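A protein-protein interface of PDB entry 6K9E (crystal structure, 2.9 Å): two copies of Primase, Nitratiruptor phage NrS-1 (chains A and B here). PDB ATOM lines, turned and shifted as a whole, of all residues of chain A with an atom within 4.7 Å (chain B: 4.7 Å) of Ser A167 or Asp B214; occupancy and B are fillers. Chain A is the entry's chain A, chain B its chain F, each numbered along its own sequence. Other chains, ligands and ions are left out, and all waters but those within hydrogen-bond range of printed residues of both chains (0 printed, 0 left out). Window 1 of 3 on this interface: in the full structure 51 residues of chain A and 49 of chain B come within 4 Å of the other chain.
The side-chain amide nitrogen of Asn A168 lies within hydrogen-bond range of the side-chain carboxylate of Asp B214 (2.9 Å).
The side-chain carboxylate (OD1) of Asp B214 is in hydrogen-bond range of the backbone NH (N) of Thr B216 (3.3 Å). O of Asp B214 sits at hydrogen-bond distance from ND2 of Asn B231 (2.9 Å). The guanidinium group of Arg B135 lies within hydrogen-bond range of the backbone carbonyl oxygen of Asp B214 (3.0 Å). O of Glu B215 lies within hydrogen-bond range of N of Asn B231 (2.6 Å). N of Asn A168 is in hydrogen-bond range of ND1 of His A189 (2.9 Å). The side-chain amide nitrogen of Asn A168 lies within hydrogen-bond range of the side-chain hydroxyl of Ser A167, 3.5 Å away.
Among the printed residues, merely in contact across the chains: Ser A167 with Asp B214 (3.6 Å), Ser A167 with Glu B215 (3.9 Å), Ser A167 with Thr B216 (3.5 Å) and Asn A168 with Thr B210 (3.9 Å).
Of chain B, only Asp B214, Glu B215 and Thr B216 come within 4 Å of Ser A167. Printed residues of chain B within 4 Å of Asn A168: Thr B210 and Asp B214. Arg B135 touches none of the printed residues of chain A. Printed residues of chain A within 4 Å of Thr B210: Asn A168. Asp B214 touches two residues of chain A. Of the printed residues of chain A, Glu B215 touches Ser A167. Of the printed residues of chain A, Thr B216 touches Ser A167. The nearest printed residue of chain B that does not touch Ser A167 is Leu B217 (6.3 Å). The nearest printed residue of chain A that does not touch Asp B214 is Ile A169 (5.5 Å). The nearest printed residue of chain A that does not touch Glu B215 is Lys A158 (4.2 Å).
Of the 10 printed residues of chain B, 4 touch a printed residue of chain A. Printed residues of chain B that touch a printed residue of chain A: Thr B210, Asp B214, Glu B215 and Thr B216. Among the printed residues, no Asp or Glu carboxylate lies within 4 Å of a Lys or Arg side-chain nitrogen of the other chain.
No position is printed for both chains. Of the 5 pairs that touch across the chains among the printed residues, none has its exchanged pair printed and touching as well.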
ATOM      1  N   VAL A 154     -18.246   1.948  -1.251  1.00  0.00           N
ATOM      2  CA  VAL A 154     -17.662   1.789  -2.580  1.00  0.00           C
ATOM      3  C   VAL A 154     -17.552   0.316  -2.974  1.00  0.00           C
ATOM      4  O   VAL A 154     -17.573  -0.006  -4.165  1.00  0.00           O
ATOM      5  CB  VAL A 154     -16.309   2.512  -2.688  1.00  0.00           C
ATOM      6  CG1 VAL A 154     -16.444   3.944  -2.180  1.00  0.00           C
ATOM      7  CG2 VAL A 154     -15.219   1.774  -1.956  1.00  0.00           C
ATOM      8  N   LYS A 158     -19.540  -1.247  -6.119  1.00  0.00           N
ATOM      9  CA  LYS A 158     -18.711  -2.038  -7.017  1.00  0.00           C
ATOM     10  C   LYS A 158     -19.366  -3.362  -7.371  1.00  0.00           C
ATOM     11  O   LYS A 158     -19.061  -3.930  -8.425  1.00  0.00           O
ATOM     12  CB  LYS A 158     -17.337  -2.279  -6.383  1.00  0.00           C
ATOM     13  CG  LYS A 158     -16.389  -3.142  -7.198  1.00  0.00           C
ATOM     14  CD  LYS A 158     -15.502  -2.325  -8.107  1.00  0.00           C
ATOM     15  CE  LYS A 158     -14.672  -3.235  -8.993  1.00  0.00           C
ATOM     16  NZ  LYS A 158     -14.421  -2.649 -10.333  1.00  0.00           N
ATOM     17  N   MET A 165     -16.997   0.415 -12.908  1.00  0.00           N
ATOM     18  CA  MET A 165     -16.495   1.190 -11.785  1.00  0.00           C
ATOM     19  C   MET A 165     -15.034   0.849 -11.541  1.00  0.00           C
ATOM     20  O   MET A 165     -14.625  -0.304 -11.692  1.00  0.00           O
ATOM     21  CB  MET A 165     -17.304   0.920 -10.513  1.00  0.00           C
ATOM     22  CG  MET A 165     -16.828   1.716  -9.311  1.00  0.00           C
ATOM     23  SD  MET A 165     -17.923   1.652  -7.890  1.00  0.00           S
ATOM     24  CE  MET A 165     -16.816   2.183  -6.588  1.00  0.00           C
ATOM     25  N   SER A 166     -14.259   1.855 -11.146  1.00  0.00           N
ATOM     26  CA  SER A 166     -12.869   1.685 -10.744  1.00  0.00           C
ATOM     27  C   SER A 166     -12.781   1.837  -9.233  1.00  0.00           C
ATOM     28  O   SER A 166     -13.222   2.851  -8.683  1.00  0.00           O
ATOM     29  CB  SER A 166     -11.970   2.704 -11.437  1.00  0.00           C
ATOM     30  OG  SER A 166     -11.666   2.281 -12.751  1.00  0.00           O
ATOM     31  N   SER A 167     -12.207   0.841  -8.565  1.00  0.00           N
ATOM     32  CA  SER A 167     -12.228   0.755  -7.112  1.00  0.00           C
ATOM     33  C   SER A 167     -10.838   0.995  -6.540  1.00  0.00           C
ATOM     34  O   SER A 167      -9.875   0.332  -6.937  1.00  0.00           O
ATOM     35  CB  SER A 167     -12.748  -0.608  -6.655  1.00  0.00           C
ATOM     36  OG  SER A 167     -13.213  -0.559  -5.318  1.00  0.00           O
ATOM     37  N   ASN A 168     -10.749   1.941  -5.603  1.00  0.00           N
ATOM     38  CA  ASN A 168      -9.532   2.197  -4.831  1.00  0.00           C
ATOM     39  C   ASN A 168      -8.347   2.500  -5.743  1.00  0.00           C
ATOM     40  O   ASN A 168      -7.287   1.878  -5.657  1.00  0.00           O
ATOM     41  CB  ASN A 168      -9.218   1.035  -3.886  1.00  0.00           C
ATOM     42  CG  ASN A 168     -10.231   0.891  -2.769  1.00  0.00           C
ATOM     43  OD1 ASN A 168     -10.409   1.796  -1.958  1.00  0.00           O
ATOM     44  ND2 ASN A 168     -10.913  -0.246  -2.731  1.00  0.00           N
ATOM     45  N   ILE A 169      -8.539   3.463  -6.635  1.00  0.00           N
ATOM     46  CA  ILE A 169      -7.447   3.975  -7.451  1.00  0.00           C
ATOM     47  C   ILE A 169      -6.601   4.899  -6.586  1.00  0.00           C
ATOM     48  O   ILE A 169      -7.101   5.891  -6.051  1.00  0.00           O
ATOM     49  CB  ILE A 169      -7.979   4.708  -8.688  1.00  0.00           C
ATOM     50  CG1 ILE A 169      -8.804   3.760  -9.556  1.00  0.00           C
ATOM     51  CG2 ILE A 169      -6.840   5.277  -9.490  1.00  0.00           C
ATOM     52  CD1 ILE A 169      -8.096   2.483  -9.895  1.00  0.00           C
ATOM     53  N   HIS A 189     -13.469   5.599  -8.274  1.00  0.00           N
ATOM     54  CA  HIS A 189     -13.210   5.849  -6.864  1.00  0.00           C
ATOM     55  C   HIS A 189     -11.716   6.034  -6.633  1.00  0.00           C
ATOM     56  O   HIS A 189     -10.907   5.203  -7.059  1.00  0.00           O
ATOM     57  CB  HIS A 189     -13.754   4.700  -6.017  1.00  0.00           C
ATOM     58  CG  HIS A 189     -13.265   4.699  -4.603  1.00  0.00           C
ATOM     59  ND1 HIS A 189     -12.572   3.638  -4.064  1.00  0.00           N
ATOM     60  CD2 HIS A 189     -13.381   5.614  -3.615  1.00  0.00           C
ATOM     61  CE1 HIS A 189     -12.271   3.904  -2.807  1.00  0.00           C
ATOM     62  NE2 HIS A 189     -12.749   5.097  -2.509  1.00  0.00           N
ATOM     63  N   ARG B 135      -9.357 -12.556   2.035  1.00  0.00           N
ATOM     64  CA  ARG B 135      -8.697 -11.338   2.469  1.00  0.00           C
ATOM     65  C   ARG B 135      -9.334 -10.856   3.760  1.00  0.00           C
ATOM     66  O   ARG B 135     -10.558 -10.745   3.854  1.00  0.00           O
ATOM     67  CB  ARG B 135      -8.770 -10.293   1.356  1.00  0.00           C
ATOM     68  CG  ARG B 135      -8.449  -8.871   1.719  1.00  0.00           C
ATOM     69  CD  ARG B 135      -8.563  -8.060   0.457  1.00  0.00           C
ATOM     70  NE  ARG B 135      -9.801  -8.338  -0.261  1.00  0.00           N
ATOM     71  CZ  ARG B 135     -10.994  -7.855   0.056  1.00  0.00           C
ATOM     72  NH1 ARG B 135     -11.129  -7.037   1.086  1.00  0.00           N
ATOM     73  NH2 ARG B 135     -12.053  -8.185  -0.673  1.00  0.00           N
ATOM     74  N   THR B 210      -4.522   1.031   1.339  1.00  0.00           N
ATOM     75  CA  THR B 210      -5.539   0.712   0.344  1.00  0.00           C
ATOM     76  C   THR B 210      -5.518  -0.761  -0.038  1.00  0.00           C
ATOM     77  O   THR B 210      -6.577  -1.375  -0.201  1.00  0.00           O
ATOM     78  CB  THR B 210      -5.322   1.569  -0.898  1.00  0.00           C
ATOM     79  OG1 THR B 210      -4.325   2.556  -0.621  1.00  0.00           O
ATOM     80  CG2 THR B 210      -6.595   2.251  -1.300  1.00  0.00           C
ATOM     81  N   TRP B 211      -4.323  -1.332  -0.210  1.00  0.00           N
ATOM     82  CA  TRP B 211      -4.208  -2.731  -0.611  1.00  0.00           C
ATOM     83  C   TRP B 211      -4.877  -3.672   0.377  1.00  0.00           C
ATOM     84  O   TRP B 211      -5.384  -4.727  -0.018  1.00  0.00           O
ATOM     85  CB  TRP B 211      -2.740  -3.117  -0.741  1.00  0.00           C
ATOM     86  CG  TRP B 211      -2.041  -2.564  -1.923  1.00  0.00           C
ATOM     87  CD1 TRP B 211      -2.604  -1.999  -3.026  1.00  0.00           C
ATOM     88  CD2 TRP B 211      -0.627  -2.535  -2.131  1.00  0.00           C
ATOM     89  NE1 TRP B 211      -1.626  -1.618  -3.910  1.00  0.00           N
ATOM     90  CE2 TRP B 211      -0.403  -1.936  -3.382  1.00  0.00           C
ATOM     91  CE3 TRP B 211       0.471  -2.957  -1.377  1.00  0.00           C
ATOM     92  CZ2 TRP B 211       0.873  -1.754  -3.899  1.00  0.00           C
ATOM     93  CZ3 TRP B 211       1.734  -2.769  -1.888  1.00  0.00           C
ATOM     94  CH2 TRP B 211       1.928  -2.172  -3.135  1.00  0.00           C
ATOM     95  N   ILE B 212      -4.889  -3.309   1.658  1.00  0.00           N
ATOM     96  CA  ILE B 212      -5.409  -4.205   2.681  1.00  0.00           C
ATOM     97  C   ILE B 212      -6.899  -4.452   2.501  1.00  0.00           C
ATOM     98  O   ILE B 212      -7.388  -5.551   2.790  1.00  0.00           O
ATOM     99  CB  ILE B 212      -5.075  -3.638   4.076  1.00  0.00           C
ATOM    100  CG1 ILE B 212      -3.561  -3.586   4.272  1.00  0.00           C
ATOM    101  CG2 ILE B 212      -5.694  -4.466   5.159  1.00  0.00           C
ATOM    102  CD1 ILE B 212      -3.130  -2.851   5.512  1.00  0.00           C
ATOM    103  N   THR B 213      -7.639  -3.468   1.992  1.00  0.00           N
ATOM    104  CA  THR B 213      -9.091  -3.570   1.905  1.00  0.00           C
ATOM    105  C   THR B 213      -9.630  -3.529   0.482  1.00  0.00           C
ATOM    106  O   THR B 213     -10.843  -3.383   0.300  1.00  0.00           O
ATOM    107  CB  THR B 213      -9.753  -2.466   2.729  1.00  0.00           C
ATOM    108  OG1 THR B 213      -9.278  -1.187   2.293  1.00  0.00           O
ATOM    109  CG2 THR B 213      -9.453  -2.658   4.203  1.00  0.00           C
ATOM    110  N   ASP B 214      -8.778  -3.634  -0.530  1.00  0.00           N
ATOM    111  CA  ASP B 214      -9.249  -3.655  -1.907  1.00  0.00           C
ATOM    112  C   ASP B 214      -9.632  -5.070  -2.314  1.00  0.00           C
ATOM    113  O   ASP B 214      -8.980  -6.038  -1.922  1.00  0.00           O
ATOM    114  CB  ASP B 214      -8.163  -3.133  -2.847  1.00  0.00           C
ATOM    115  CG  ASP B 214      -8.720  -2.324  -4.001  1.00  0.00           C
ATOM    116  OD1 ASP B 214      -9.931  -2.429  -4.284  1.00  0.00           O
ATOM    117  OD2 ASP B 214      -7.932  -1.599  -4.647  1.00  0.00           O
ATOM    118  N   GLU B 215     -10.684  -5.186  -3.119  1.00  0.00           N
ATOM    119  CA  GLU B 215     -10.990  -6.450  -3.772  1.00  0.00           C
ATOM    120  C   GLU B 215     -10.281  -6.557  -5.103  1.00  0.00           C
ATOM    121  O   GLU B 215     -10.096  -7.667  -5.611  1.00  0.00           O
ATOM    122  CB  GLU B 215     -12.492  -6.620  -4.024  1.00  0.00           C
ATOM    123  CG  GLU B 215     -13.376  -6.135  -2.985  1.00  0.00           C
ATOM    124  CD  GLU B 215     -13.746  -4.757  -3.182  1.00  0.00           C
ATOM    125  OE1 GLU B 215     -13.655  -4.305  -4.187  1.00  0.00           O
ATOM    126  OE2 GLU B 215     -14.094  -4.103  -2.328  1.00  0.00           O
ATOM    127  N   THR B 216      -9.893  -5.421  -5.670  1.00  0.00           N
ATOM    128  CA  THR B 216      -9.421  -5.346  -7.038  1.00  0.00           C
ATOM    129  C   THR B 216      -8.061  -4.659  -7.085  1.00  0.00           C
ATOM    130  O   THR B 216      -7.865  -3.605  -6.473  1.00  0.00           O
ATOM    131  CB  THR B 216     -10.464  -4.599  -7.888  1.00  0.00           C
ATOM    132  OG1 THR B 216     -10.327  -4.980  -9.250  1.00  0.00           O
ATOM    133  CG2 THR B 216     -10.353  -3.065  -7.774  1.00  0.00           C
ATOM    134  N   LEU B 217      -7.100  -5.301  -7.750  1.00  0.00           N
ATOM    135  CA  LEU B 217      -5.814  -4.695  -8.066  1.00  0.00           C
ATOM    136  C   LEU B 217      -5.539  -4.840  -9.554  1.00  0.00           C
ATOM    137  O   LEU B 217      -5.967  -5.808 -10.184  1.00  0.00           O
ATOM    138  CB  LEU B 217      -4.671  -5.330  -7.255  1.00  0.00           C
ATOM    139  CG  LEU B 217      -4.897  -5.521  -5.757  1.00  0.00           C
ATOM    140  CD1 LEU B 217      -3.732  -6.244  -5.117  1.00  0.00           C
ATOM    141  CD2 LEU B 217      -5.101  -4.175  -5.087  1.00  0.00           C
ATOM    142  N   ASN B 231      -8.353  -9.591  -5.199  1.00  0.00           N
ATOM    143  CA  ASN B 231      -7.252  -9.426  -4.255  1.00  0.00           C
ATOM    144  C   ASN B 231      -7.515 -10.310  -3.044  1.00  0.00           C
ATOM    145  O   ASN B 231      -8.563 -10.201  -2.399  1.00  0.00           O
ATOM    146  CB  ASN B 231      -7.084  -7.959  -3.847  1.00  0.00           C
ATOM    147  CG  ASN B 231      -6.087  -7.762  -2.704  1.00  0.00           C
ATOM    148  OD1 ASN B 231      -5.264  -8.630  -2.428  1.00  0.00           O
ATOM    149  ND2 ASN B 231      -6.131  -6.592  -2.071  1.00  0.00           N
